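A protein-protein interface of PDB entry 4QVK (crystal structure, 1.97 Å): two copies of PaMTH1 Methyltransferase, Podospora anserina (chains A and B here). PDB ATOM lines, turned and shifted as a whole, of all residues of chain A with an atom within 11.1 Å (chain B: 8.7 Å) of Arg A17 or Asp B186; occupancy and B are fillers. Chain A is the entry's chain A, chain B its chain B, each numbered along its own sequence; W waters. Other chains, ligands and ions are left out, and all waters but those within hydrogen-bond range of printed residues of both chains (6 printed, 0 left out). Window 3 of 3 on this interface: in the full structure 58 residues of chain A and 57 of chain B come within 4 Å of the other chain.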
ATOM      1  N   PRO A   9      -1.325 -33.180  19.683  1.00  0.00           N
ATOM      2  CA  PRO A   9      -0.309 -33.660  20.631  1.00  0.00           C
ATOM      3  C   PRO A   9       1.075 -33.100  20.282  1.00  0.00           C
ATOM      4  O   PRO A   9       1.481 -33.141  19.117  1.00  0.00           O
ATOM      5  CB  PRO A   9      -0.343 -35.183  20.453  1.00  0.00           C
ATOM      6  CG  PRO A   9      -0.744 -35.350  18.971  1.00  0.00           C
ATOM      7  CD  PRO A   9      -1.687 -34.195  18.663  1.00  0.00           C
ATOM      8  N   PHE A  10       1.758 -32.521  21.258  1.00  0.00           N
ATOM      9  CA  PHE A  10       3.125 -31.997  21.088  1.00  0.00           C
ATOM     10  C   PHE A  10       3.979 -32.489  22.250  1.00  0.00           C
ATOM     11  O   PHE A  10       3.441 -32.590  23.375  1.00  0.00           O
ATOM     12  CB  PHE A  10       3.165 -30.457  21.103  1.00  0.00           C
ATOM     13  CG  PHE A  10       2.505 -29.811  19.957  1.00  0.00           C
ATOM     14  CD1 PHE A  10       3.013 -29.963  18.676  1.00  0.00           C
ATOM     15  CD2 PHE A  10       1.396 -28.995  20.157  1.00  0.00           C
ATOM     16  CE1 PHE A  10       2.395 -29.336  17.590  1.00  0.00           C
ATOM     17  CE2 PHE A  10       0.789 -28.378  19.122  1.00  0.00           C
ATOM     18  CZ  PHE A  10       1.282 -28.546  17.808  1.00  0.00           C
ATOM     19  N   ASN A  11       5.277 -32.755  22.030  1.00  0.00           N
ATOM     20  CA  ASN A  11       6.165 -32.981  23.173  1.00  0.00           C
ATOM     21  C   ASN A  11       6.533 -31.594  23.759  1.00  0.00           C
ATOM     22  O   ASN A  11       6.060 -30.552  23.260  1.00  0.00           O
ATOM     23  CB  ASN A  11       7.406 -33.822  22.814  1.00  0.00           C
ATOM     24  CG  ASN A  11       8.310 -33.181  21.748  1.00  0.00           C
ATOM     25  OD1 ASN A  11       8.283 -31.975  21.498  1.00  0.00           O
ATOM     26  ND2 ASN A  11       9.126 -34.005  21.119  1.00  0.00           N
ATOM     27  N   GLU A  12       7.336 -31.567  24.817  1.00  0.00           N
ATOM     28  CA  GLU A  12       7.574 -30.292  25.488  1.00  0.00           C
ATOM     29  C   GLU A  12       8.303 -29.325  24.572  1.00  0.00           C
ATOM     30  O   GLU A  12       7.903 -28.176  24.433  1.00  0.00           O
ATOM     31  CB  GLU A  12       8.398 -30.475  26.758  1.00  0.00           C
ATOM     32  CG  GLU A  12       7.756 -31.281  27.820  1.00  0.00           C
ATOM     33  CD  GLU A  12       8.738 -31.563  28.932  1.00  0.00           C
ATOM     34  OE1 GLU A  12       9.418 -32.615  28.884  1.00  0.00           O
ATOM     35  OE2 GLU A  12       8.856 -30.696  29.831  1.00  0.00           O
ATOM     36  N   GLU A  13       9.383 -29.804  23.955  1.00  0.00           N
ATOM     37  CA  GLU A  13      10.202 -28.961  23.091  1.00  0.00           C
ATOM     38  C   GLU A  13       9.331 -28.356  21.986  1.00  0.00           C
ATOM     39  O   GLU A  13       9.336 -27.140  21.729  1.00  0.00           O
ATOM     40  CB  GLU A  13      11.355 -29.773  22.508  1.00  0.00           C
ATOM     41  CG  GLU A  13      12.208 -29.003  21.532  1.00  0.00           C
ATOM     42  CD  GLU A  13      13.435 -29.774  21.104  1.00  0.00           C
ATOM     43  OE1 GLU A  13      13.981 -30.548  21.921  1.00  0.00           O
ATOM     44  OE2 GLU A  13      13.861 -29.613  19.938  1.00  0.00           O
ATOM     45  N   THR A  14       8.508 -29.194  21.376  1.00  0.00           N
ATOM     46  CA  THR A  14       7.737 -28.726  20.230  1.00  0.00           C
ATOM     47  C   THR A  14       6.572 -27.815  20.646  1.00  0.00           C
ATOM     48  O   THR A  14       6.237 -26.862  19.929  1.00  0.00           O
ATOM     49  CB  THR A  14       7.236 -29.915  19.400  1.00  0.00           C
ATOM     50  OG1 THR A  14       8.376 -30.666  18.955  1.00  0.00           O
ATOM     51  CG2 THR A  14       6.464 -29.419  18.168  1.00  0.00           C
ATOM     52  N   ALA A  15       5.950 -28.093  21.790  1.00  0.00           N
ATOM     53  CA  ALA A  15       4.890 -27.228  22.296  1.00  0.00           C
ATOM     54  C   ALA A  15       5.490 -25.843  22.475  1.00  0.00           C
ATOM     55  O   ALA A  15       4.919 -24.830  22.021  1.00  0.00           O
ATOM     56  CB  ALA A  15       4.324 -27.751  23.625  1.00  0.00           C
ATOM     57  N   ASP A  16       6.630 -25.789  23.160  1.00  0.00           N
ATOM     58  CA  ASP A  16       7.304 -24.511  23.323  1.00  0.00           C
ATOM     59  C   ASP A  16       7.620 -23.825  21.985  1.00  0.00           C
ATOM     60  O   ASP A  16       7.461 -22.599  21.813  1.00  0.00           O
ATOM     61  CB  ASP A  16       8.566 -24.693  24.139  1.00  0.00           C
ATOM     62  CG  ASP A  16       8.285 -24.639  25.602  1.00  0.00           C
ATOM     63  OD1 ASP A  16       7.085 -24.510  25.970  1.00  0.00           O
ATOM     64  OD2 ASP A  16       9.244 -24.672  26.382  1.00  0.00           O
ATOM     65  N   ARG A  17       8.073 -24.599  21.026  1.00  0.00           N
ATOM     66  CA  ARG A  17       8.402 -24.011  19.728  1.00  0.00           C
ATOM     67  C   ARG A  17       7.147 -23.433  19.017  1.00  0.00           C
ATOM     68  O   ARG A  17       7.177 -22.336  18.432  1.00  0.00           O
ATOM     69  CB  ARG A  17       9.078 -25.070  18.871  1.00  0.00           C
ATOM     70  CG  ARG A  17       9.642 -24.578  17.563  1.00  0.00           C
ATOM     71  CD  ARG A  17      10.182 -25.782  16.804  1.00  0.00           C
ATOM     72  NE  ARG A  17      10.553 -25.431  15.441  1.00  0.00           N
ATOM     73  CZ  ARG A  17      10.944 -26.342  14.550  1.00  0.00           C
ATOM     74  NH1 ARG A  17      10.983 -27.614  14.898  1.00  0.00           N
ATOM     75  NH2 ARG A  17      11.287 -25.976  13.327  1.00  0.00           N
ATOM     76  N   VAL A  18       6.046 -24.180  19.059  1.00  0.00           N
ATOM     77  CA  VAL A  18       4.804 -23.699  18.487  1.00  0.00           C
ATOM     78  C   VAL A  18       4.294 -22.448  19.228  1.00  0.00           C
ATOM     79  O   VAL A  18       3.763 -21.562  18.580  1.00  0.00           O
ATOM     80  CB  VAL A  18       3.747 -24.819  18.474  1.00  0.00           C
ATOM     81  CG1 VAL A  18       2.416 -24.309  17.986  1.00  0.00           C
ATOM     82  CG2 VAL A  18       4.214 -25.955  17.536  1.00  0.00           C
ATOM     83  N   SER A  19       4.492 -22.346  20.554  1.00  0.00           N
ATOM     84  CA  SER A  19       4.134 -21.122  21.261  1.00  0.00           C
ATOM     85  C   SER A  19       4.876 -19.937  20.689  1.00  0.00           C
ATOM     86  O   SER A  19       4.294 -18.887  20.482  1.00  0.00           O
ATOM     87  CB  SER A  19       4.462 -21.188  22.764  1.00  0.00           C
ATOM     88  OG  SER A  19       3.660 -22.173  23.349  1.00  0.00           O
ATOM     89  N   ALA A  20       6.178 -20.107  20.474  1.00  0.00           N
ATOM     90  CA  ALA A  20       7.005 -19.004  20.009  1.00  0.00           C
ATOM     91  C   ALA A  20       6.556 -18.628  18.584  1.00  0.00           C
ATOM     92  O   ALA A  20       6.652 -17.471  18.183  1.00  0.00           O
ATOM     93  CB  ALA A  20       8.481 -19.373  20.041  1.00  0.00           C
ATOM     94  N   TYR A  21       6.071 -19.615  17.835  1.00  0.00           N
ATOM     95  CA  TYR A  21       5.599 -19.355  16.475  1.00  0.00           C
ATOM     96  C   TYR A  21       4.343 -18.468  16.521  1.00  0.00           C
ATOM     97  O   TYR A  21       4.224 -17.503  15.762  1.00  0.00           O
ATOM     98  CB  TYR A  21       5.301 -20.659  15.738  1.00  0.00           C
ATOM     99  CG  TYR A  21       4.932 -20.405  14.306  1.00  0.00           C
ATOM    100  CD1 TYR A  21       5.901 -20.337  13.314  1.00  0.00           C
ATOM    101  CD2 TYR A  21       3.615 -20.227  13.949  1.00  0.00           C
ATOM    102  CE1 TYR A  21       5.549 -20.100  12.008  1.00  0.00           C
ATOM    103  CE2 TYR A  21       3.247 -19.992  12.615  1.00  0.00           C
ATOM    104  CZ  TYR A  21       4.204 -19.948  11.677  1.00  0.00           C
ATOM    105  OH  TYR A  21       3.827 -19.667  10.393  1.00  0.00           O
ATOM    106  N   CYS A  22       3.450 -18.775  17.450  1.00  0.00           N
ATOM    107  CA  CYS A  22       2.257 -17.952  17.662  1.00  0.00           C
ATOM    108  C   CYS A  22       2.617 -16.526  18.046  1.00  0.00           C
ATOM    109  O   CYS A  22       2.035 -15.561  17.495  1.00  0.00           O
ATOM    110  CB  CYS A  22       1.335 -18.591  18.726  1.00  0.00           C
ATOM    111  SG  CYS A  22       0.641 -20.196  18.193  1.00  0.00           S
ATOM    112  N   GLU A  23       3.608 -16.372  18.928  1.00  0.00           N
ATOM    113  CA  GLU A  23       4.035 -15.040  19.312  1.00  0.00           C
ATOM    114  C   GLU A  23       4.622 -14.296  18.120  1.00  0.00           C
ATOM    115  O   GLU A  23       4.372 -13.099  17.939  1.00  0.00           O
ATOM    116  CB  GLU A  23       5.052 -15.072  20.471  1.00  0.00           C
ATOM    117  CG  GLU A  23       4.430 -15.618  21.750  1.00  0.00           C
ATOM    118  CD  GLU A  23       5.301 -15.384  22.991  1.00  0.00           C
ATOM    119  OE1 GLU A  23       6.345 -14.682  22.893  1.00  0.00           O
ATOM    120  OE2 GLU A  23       4.901 -15.868  24.081  1.00  0.00           O
ATOM    121  N   LYS A  24       5.429 -14.987  17.324  1.00  0.00           N
ATOM    122  CA  LYS A  24       6.067 -14.323  16.167  1.00  0.00           C
ATOM    123  C   LYS A  24       4.989 -13.826  15.214  1.00  0.00           C
ATOM    124  O   LYS A  24       5.084 -12.762  14.657  1.00  0.00           O
ATOM    125  CB  LYS A  24       6.984 -15.291  15.437  1.00  0.00           C
ATOM    126  CG  LYS A  24       7.749 -14.720  14.242  1.00  0.00           C
ATOM    127  CD  LYS A  24       8.574 -15.854  13.620  1.00  0.00           C
ATOM    128  CE  LYS A  24       9.650 -15.323  12.703  1.00  0.00           C
ATOM    129  NZ  LYS A  24       8.997 -14.623  11.541  1.00  0.00           N
ATOM    130  N   ASN A  25       3.929 -14.604  15.088  1.00  0.00           N
ATOM    131  CA  ASN A  25       2.873 -14.343  14.100  1.00  0.00           C
ATOM    132  C   ASN A  25       1.573 -13.814  14.691  1.00  0.00           C
ATOM    133  O   ASN A  25       0.479 -14.057  14.130  1.00  0.00           O
ATOM    134  CB  ASN A  25       2.590 -15.620  13.301  1.00  0.00           C
ATOM    135  CG  ASN A  25       3.743 -15.974  12.389  1.00  0.00           C
ATOM    136  OD1 ASN A  25       3.951 -15.315  11.372  1.00  0.00           O
ATOM    137  ND2 ASN A  25       4.533 -16.980  12.773  1.00  0.00           N
ATOM    138  N   SER A  26       1.726 -13.120  15.829  1.00  0.00           N
ATOM    139  CA  SER A  26       0.659 -12.367  16.483  1.00  0.00           C
ATOM    140  C   SER A  26       1.265 -11.029  16.845  1.00  0.00           C
ATOM    141  O   SER A  26       2.442 -10.970  17.213  1.00  0.00           O
ATOM    142  CB  SER A  26       0.143 -13.058  17.744  1.00  0.00           C
ATOM    143  OG  SER A  26      -0.268 -14.398  17.501  1.00  0.00           O
ATOM    144  N   LEU A  54       2.215 -14.245  24.775  1.00  0.00           N
ATOM    145  CA  LEU A  54       1.094 -14.570  23.901  1.00  0.00           C
ATOM    146  C   LEU A  54      -0.236 -14.373  24.597  1.00  0.00           C
ATOM    147  O   LEU A  54      -1.183 -13.838  24.013  1.00  0.00           O
ATOM    148  CB  LEU A  54       1.199 -16.003  23.417  1.00  0.00           C
ATOM    149  CG  LEU A  54       0.111 -16.456  22.433  1.00  0.00           C
ATOM    150  CD1 LEU A  54       0.185 -15.599  21.152  1.00  0.00           C
ATOM    151  CD2 LEU A  54       0.386 -17.915  22.117  1.00  0.00           C
ATOM    152  N   LEU B   4       9.671 -20.960  28.464  1.00  0.00           N
ATOM    153  CA  LEU B   4       8.375 -21.624  28.580  1.00  0.00           C
ATOM    154  C   LEU B   4       7.232 -20.897  27.851  1.00  0.00           C
ATOM    155  O   LEU B   4       7.200 -19.654  27.779  1.00  0.00           O
ATOM    156  CB  LEU B   4       8.005 -21.811  30.053  1.00  0.00           C
ATOM    157  CG  LEU B   4       8.130 -23.245  30.587  1.00  0.00           C
ATOM    158  CD1 LEU B   4       8.068 -23.158  32.096  1.00  0.00           C
ATOM    159  CD2 LEU B   4       7.065 -24.203  30.040  1.00  0.00           C
ATOM    160  N   GLY B   5       6.297 -21.705  27.336  1.00  0.00           N
ATOM    161  CA  GLY B   5       5.285 -21.248  26.408  1.00  0.00           C
ATOM    162  C   GLY B   5       3.862 -21.405  26.893  1.00  0.00           C
ATOM    163  O   GLY B   5       3.618 -21.641  28.066  1.00  0.00           O
ATOM    164  N   SER B   6       2.927 -21.277  25.960  1.00  0.00           N
ATOM    165  CA  SER B   6       1.495 -21.234  26.227  1.00  0.00           C
ATOM    166  C   SER B   6       0.742 -22.498  25.851  1.00  0.00           C
ATOM    167  O   SER B   6      -0.485 -22.484  25.761  1.00  0.00           O
ATOM    168  CB  SER B   6       0.860 -20.081  25.451  1.00  0.00           C
ATOM    169  OG  SER B   6       1.685 -18.946  25.492  1.00  0.00           O
ATOM    170  N   ILE B   7       1.473 -23.566  25.572  1.00  0.00           N
ATOM    171  CA  ILE B   7       0.874 -24.786  25.074  1.00  0.00           C
ATOM    172  C   ILE B   7       1.283 -25.953  25.954  1.00  0.00           C
ATOM    173  O   ILE B   7       2.454 -26.195  26.153  1.00  0.00           O
ATOM    174  CB  ILE B   7       1.301 -25.041  23.611  1.00  0.00           C
ATOM    175  CG1 ILE B   7       0.805 -23.871  22.751  1.00  0.00           C
ATOM    176  CG2 ILE B   7       0.689 -26.390  23.082  1.00  0.00           C
ATOM    177  CD1 ILE B   7       1.270 -23.894  21.227  1.00  0.00           C
ATOM    178  N   PHE B 177      -2.369 -24.333  11.633  1.00  0.00           N
ATOM    179  CA  PHE B 177      -1.166 -25.081  12.059  1.00  0.00           C
ATOM    180  C   PHE B 177      -0.785 -26.226  11.112  1.00  0.00           C
ATOM    181  O   PHE B 177       0.322 -26.758  11.185  1.00  0.00           O
ATOM    182  CB  PHE B 177      -1.351 -25.700  13.449  1.00  0.00           C
ATOM    183  CG  PHE B 177      -1.228 -24.734  14.598  1.00  0.00           C
ATOM    184  CD1 PHE B 177      -0.749 -23.448  14.427  1.00  0.00           C
ATOM    185  CD2 PHE B 177      -1.589 -25.152  15.874  1.00  0.00           C
ATOM    186  CE1 PHE B 177      -0.635 -22.566  15.547  1.00  0.00           C
ATOM    187  CE2 PHE B 177      -1.481 -24.318  16.963  1.00  0.00           C
ATOM    188  CZ  PHE B 177      -0.991 -23.008  16.808  1.00  0.00           C
ATOM    189  N   ARG B 179      -1.541 -29.283  11.327  1.00  0.00           N
ATOM    190  CA  ARG B 179      -1.162 -30.376  12.238  1.00  0.00           C
ATOM    191  C   ARG B 179       0.153 -30.139  12.973  1.00  0.00           C
ATOM    192  O   ARG B 179       0.620 -31.028  13.693  1.00  0.00           O
ATOM    193  CB  ARG B 179      -1.061 -31.723  11.506  1.00  0.00           C
ATOM    194  CG  ARG B 179      -2.339 -32.128  10.766  1.00  0.00           C
ATOM    195  CD  ARG B 179      -3.437 -32.598  11.707  1.00  0.00           C
ATOM    196  NE  ARG B 179      -4.460 -33.344  10.973  1.00  0.00           N
ATOM    197  CZ  ARG B 179      -5.491 -32.755  10.372  1.00  0.00           C
ATOM    198  NH1 ARG B 179      -5.641 -31.437  10.479  1.00  0.00           N
ATOM    199  NH2 ARG B 179      -6.391 -33.463   9.698  1.00  0.00           N
ATOM    200  N   GLY B 180       0.718 -28.944  12.787  1.00  0.00           N
ATOM    201  CA  GLY B 180       1.992 -28.553  13.366  1.00  0.00           C
ATOM    202  C   GLY B 180       2.998 -28.273  12.251  1.00  0.00           C
ATOM    203  O   GLY B 180       4.008 -27.625  12.460  1.00  0.00           O
ATOM    204  N   LEU B 181       2.706 -28.734  11.040  1.00  0.00           N
ATOM    205  CA  LEU B 181       3.691 -28.684   9.964  1.00  0.00           C
ATOM    206  C   LEU B 181       3.876 -27.263   9.444  1.00  0.00           C
ATOM    207  O   LEU B 181       4.849 -26.987   8.755  1.00  0.00           O
ATOM    208  CB  LEU B 181       3.296 -29.635   8.823  1.00  0.00           C
ATOM    209  CG  LEU B 181       3.300 -31.097   9.292  1.00  0.00           C
ATOM    210  CD1 LEU B 181       3.131 -32.135   8.121  1.00  0.00           C
ATOM    211  CD2 LEU B 181       4.593 -31.367  10.063  1.00  0.00           C
ATOM    212  N   THR B 182       2.955 -26.361   9.789  1.00  0.00           N
ATOM    213  CA  THR B 182       3.140 -24.929   9.474  1.00  0.00           C
ATOM    214  C   THR B 182       4.419 -24.402  10.146  1.00  0.00           C
ATOM    215  O   THR B 182       5.164 -23.598   9.591  1.00  0.00           O
ATOM    216  CB  THR B 182       1.948 -24.107   9.937  1.00  0.00           C
ATOM    217  OG1 THR B 182       0.804 -24.499   9.168  1.00  0.00           O
ATOM    218  CG2 THR B 182       2.213 -22.609   9.754  1.00  0.00           C
ATOM    219  N   ILE B 183       4.660 -24.880  11.359  1.00  0.00           N
ATOM    220  CA  ILE B 183       5.779 -24.411  12.173  1.00  0.00           C
ATOM    221  C   ILE B 183       7.079 -25.083  11.691  1.00  0.00           C
ATOM    222  O   ILE B 183       8.151 -24.459  11.598  1.00  0.00           O
ATOM    223  CB  ILE B 183       5.537 -24.705  13.677  1.00  0.00           C
ATOM    224  CG1 ILE B 183       4.325 -23.915  14.203  1.00  0.00           C
ATOM    225  CG2 ILE B 183       6.782 -24.427  14.490  1.00  0.00           C
ATOM    226  CD1 ILE B 183       2.928 -24.665  14.009  1.00  0.00           C
ATOM    227  N   GLY B 184       6.991 -26.357  11.341  1.00  0.00           N
ATOM    228  CA  GLY B 184       8.160 -27.006  10.752  1.00  0.00           C
ATOM    229  C   GLY B 184       7.943 -28.491  10.512  1.00  0.00           C
ATOM    230  O   GLY B 184       7.048 -29.082  11.109  1.00  0.00           O
ATOM    231  N   PRO B 185       8.788 -29.112   9.673  1.00  0.00           N
ATOM    232  CA  PRO B 185       8.498 -30.477   9.205  1.00  0.00           C
ATOM    233  C   PRO B 185       8.577 -31.499  10.329  1.00  0.00           C
ATOM    234  O   PRO B 185       8.077 -32.603  10.149  1.00  0.00           O
ATOM    235  CB  PRO B 185       9.595 -30.759   8.181  1.00  0.00           C
ATOM    236  CG  PRO B 185      10.296 -29.459   7.936  1.00  0.00           C
ATOM    237  CD  PRO B 185      10.029 -28.566   9.110  1.00  0.00           C
ATOM    238  N   ASP B 186       9.225 -31.157  11.451  1.00  0.00           N
ATOM    239  CA  ASP B 186       9.469 -32.150  12.486  1.00  0.00           C
ATOM    240  C   ASP B 186       8.472 -31.995  13.616  1.00  0.00           C
ATOM    241  O   ASP B 186       8.585 -32.647  14.640  1.00  0.00           O
ATOM    242  CB  ASP B 186      10.894 -32.055  13.008  1.00  0.00           C
ATOM    243  CG  ASP B 186      11.213 -30.705  13.613  1.00  0.00           C
ATOM    244  OD1 ASP B 186      10.663 -29.664  13.136  1.00  0.00           O
ATOM    245  OD2 ASP B 186      12.034 -30.701  14.564  1.00  0.00           O
ATOM    246  N   CYS B 187       7.470 -31.158  13.397  1.00  0.00           N
ATOM    247  CA  CYS B 187       6.538 -30.791  14.448  1.00  0.00           C
ATOM    248  C   CYS B 187       5.307 -31.658  14.588  1.00  0.00           C
ATOM    249  O   CYS B 187       4.443 -31.329  15.396  1.00  0.00           O
ATOM    250  CB  CYS B 187       6.080 -29.343  14.238  1.00  0.00           C
ATOM    251  SG  CYS B 187       7.421 -28.191  14.605  1.00  0.00           S
ATOM    252  N   ALA B 188       5.217 -32.736  13.797  1.00  0.00           N
ATOM    253  CA  ALA B 188       4.080 -33.630  13.883  1.00  0.00           C
ATOM    254  C   ALA B 188       4.474 -35.087  13.656  1.00  0.00           C
ATOM    255  O   ALA B 188       4.025 -35.710  12.688  1.00  0.00           O
ATOM    256  CB  ALA B 188       2.981 -33.197  12.851  1.00  0.00           C
ATOM    257  N   PRO B 189       5.311 -35.646  14.534  1.00  0.00           N
ATOM    258  CA  PRO B 189       5.811 -36.992  14.222  1.00  0.00           C
ATOM    259  C   PRO B 189       4.729 -38.079  14.289  1.00  0.00           C
ATOM    260  O   PRO B 189       4.914 -39.163  13.744  1.00  0.00           O
ATOM    261  CB  PRO B 189       6.882 -37.224  15.293  1.00  0.00           C
ATOM    262  CG  PRO B 189       6.519 -36.269  16.413  1.00  0.00           C
ATOM    263  CD  PRO B 189       5.963 -35.067  15.726  1.00  0.00           C
ATOM    264  N   TRP B 190       3.601 -37.768  14.915  1.00  0.00           N
ATOM    265  CA  TRP B 190       2.527 -38.747  15.049  1.00  0.00           C
ATOM    266  C   TRP B 190       1.672 -38.878  13.776  1.00  0.00           C
ATOM    267  O   TRP B 190       0.894 -39.816  13.624  1.00  0.00           O
ATOM    268  CB  TRP B 190       1.628 -38.352  16.218  1.00  0.00           C
ATOM    269  CG  TRP B 190       1.128 -36.962  16.042  1.00  0.00           C
ATOM    270  CD1 TRP B 190       1.757 -35.822  16.436  1.00  0.00           C
ATOM    271  CD2 TRP B 190      -0.086 -36.550  15.382  1.00  0.00           C
ATOM    272  NE1 TRP B 190       1.011 -34.719  16.081  1.00  0.00           N
ATOM    273  CE2 TRP B 190      -0.129 -35.141  15.439  1.00  0.00           C
ATOM    274  CE3 TRP B 190      -1.136 -37.242  14.745  1.00  0.00           C
ATOM    275  CZ2 TRP B 190      -1.179 -34.401  14.876  1.00  0.00           C
ATOM    276  CZ3 TRP B 190      -2.188 -36.510  14.212  1.00  0.00           C
ATOM    277  CH2 TRP B 190      -2.206 -35.105  14.278  1.00  0.00           C
ATOM    278  N   ARG B 196       0.927 -36.823   5.164  1.00  0.00           N
ATOM    279  CA  ARG B 196       1.985 -35.883   5.553  1.00  0.00           C
ATOM    280  C   ARG B 196       2.433 -34.946   4.399  1.00  0.00           C
ATOM    281  O   ARG B 196       2.605 -33.733   4.622  1.00  0.00           O
ATOM    282  CB  ARG B 196       3.185 -36.666   6.116  1.00  0.00           C
ATOM    283  CG  ARG B 196       4.412 -35.820   6.467  1.00  0.00           C
ATOM    284  CD  ARG B 196       5.506 -36.719   7.012  1.00  0.00           C
ATOM    285  NE  ARG B 196       5.074 -37.458   8.190  1.00  0.00           N
ATOM    286  CZ  ARG B 196       5.013 -36.909   9.400  1.00  0.00           C
ATOM    287  NH1 ARG B 196       5.340 -35.630   9.560  1.00  0.00           N
ATOM    288  NH2 ARG B 196       4.607 -37.615  10.444  1.00  0.00           N
ATOM    289  N   ASN B 200       2.166 -30.962   4.822  1.00  0.00           N
ATOM    290  CA  ASN B 200       3.405 -30.215   4.687  1.00  0.00           C
ATOM    291  C   ASN B 200       3.228 -29.099   3.651  1.00  0.00           C
ATOM    292  O   ASN B 200       3.652 -27.955   3.864  1.00  0.00           O
ATOM    293  CB  ASN B 200       4.554 -31.143   4.297  1.00  0.00           C
ATOM    294  CG  ASN B 200       5.879 -30.593   4.701  1.00  0.00           C
ATOM    295  OD1 ASN B 200       6.141 -30.363   5.898  1.00  0.00           O
ATOM    296  ND2 ASN B 200       6.733 -30.366   3.729  1.00  0.00           N
HETATM  297  O   HOH W   1       7.992 -33.030  17.393  1.00  0.00           O
HETATM  298  O   HOH W   2       0.751 -32.177  16.278  1.00  0.00           O
HETATM  299  O   HOH W   3       4.462 -18.333  24.407  1.00  0.00           O
HETATM  300  O   HOH W   4       3.640 -33.149  17.547  1.00  0.00           O
HETATM  301  O   HOH W   5      11.777 -27.994  11.589  1.00  0.00           O
HETATM  302  O   HOH W   6       4.360 -24.437  25.463  1.00  0.00           O
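Arg A17 touches just these residues of chain B: Ile B183, Asp B186 and Cys B187.
Of chain A, only Arg A17 comes within 4 Å of Asp B186.
No residue of chain A comes within 4 Å of Ala B188.
Of the printed residues of chain A, Trp B190 touches Pro A9.
Of the printed residues of chain B, Val A18 touches Ile B7 (3.5 Å), Phe B177 (3.8 Å) and Ile B183 (3.9 Å).
The nearest residue of chain B that does not touch Arg A17 is Gly B184 (4.2 Å).
The nearest residue of chain A that does not touch Asp B186 is Thr A14 (4.8 Å).
Water W3 bridges OE2 of Glu A23 (2.5 Å) and OG of Ser B6 (3.0 Å).
Water W5 lies within hydrogen-bond range of OD1 of Asp B186 (2.5 Å) and NH2 of Arg A17 (2.7 Å).
Water W2 lies within hydrogen-bond range of NE1 of Trp B190 (2.6 Å), O of Arg B179 (2.8 Å) and O of Pro A9 (3.1 Å).
Water W4 lies within hydrogen-bond range of the backbone carbonyl oxygen (O) of Pro A9 (2.7 Å), the backbone carbonyl oxygen (O) of Cys B187 (2.9 Å) and the indole nitrogen (NE1) of Trp B190 (3.4 Å).
Water W6 lies within hydrogen-bond range of the backbone carbonyl oxygen of Ile B7 (2.7 Å), the side-chain carboxylate of Asp A16 (2.8 Å) and the side-chain hydroxyl of Ser A19 (3.2 Å).
Water W1 lies within hydrogen-bond range of O of Asp B186 (2.8 Å) and OG1 of Thr A14 (2.9 Å).
O of Cys A22 lies within hydrogen-bond range of OG of Ser A26.
O of Gly B184 sits close to SG of Cys B187.
The backbone carbonyl oxygen of Ala A15 lies within hydrogen-bond range of the side-chain hydroxyl of Ser A19 (3.2 Å).
The side-chain carboxylate (OE2) of Glu A23 is in hydrogen-bond range of the backbone NH (N) of Leu A54.
The backbone NH (N) of Thr A14 lies within hydrogen-bond range of the side-chain amide oxygen (OD1) of Asn A11.
SG of Cys A22 lies within hydrogen-bond range of O of Val A18, at 3.4 Å.
No position is printed for both chains.
Of the 19 printed residues of chain B, 10 touch a printed residue of chain A.
Printed residues of chain B that touch a printed residue of chain A: Leu B4, Gly B5, Ser B6, Ile B7, Phe B177, Thr B182, Ile B183, Asp B186, Cys B187 and Trp B190.
Hydrophobic or aromatic side chains of chain B within 4 Å of the printed part of chain A: Ile B7, Phe B177, Ile B183 and Trp B190.
Of the 19 printed residues of chain A, 11 touch a printed residue of chain B.
Phe A10 touches Ile B7 (CD2 to CG2, 3.98 Å).
O of Cys B187 touches CE1 of Phe A10, 3.6 Å away.
Thr A14 touches Cys B187.
Ile B7 touches Ala A15.
Arg A17 touches Ile B183.
Ile B7 touches Val A18.
CG1 of Ile B183 touches CG2 of Val A18, 3.9 Å away.
Gly B5 touches Ser A19 (CA to OG, 3.6 Å).
Tyr A21 touches Ile B183.
Cys A22 touches Phe B177.
OG of Ser A19 sits close to N of Ile B7 (3.4 Å).
The indole nitrogen (NE1) of Trp B190 sits close to the backbone carbonyl oxygen (O) of Pro A9 (3.5 Å).
The side-chain sulfur of Cys B187 sits at hydrogen-bond distance from the guanidinium group of Arg A17 (3.6 Å).
The backbone NH (N) of Ser B6 sits at hydrogen-bond distance from the side-chain hydroxyl (OG) of Ser A19 (2.9 Å).
OD1 of Asp A16 is in hydrogen-bond range of N of Gly B5 (3.2 Å).
The guanidinium group of Arg A17 is in salt-bridge range of the side-chain carboxylate of Asp B186, at 2.7 Å.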
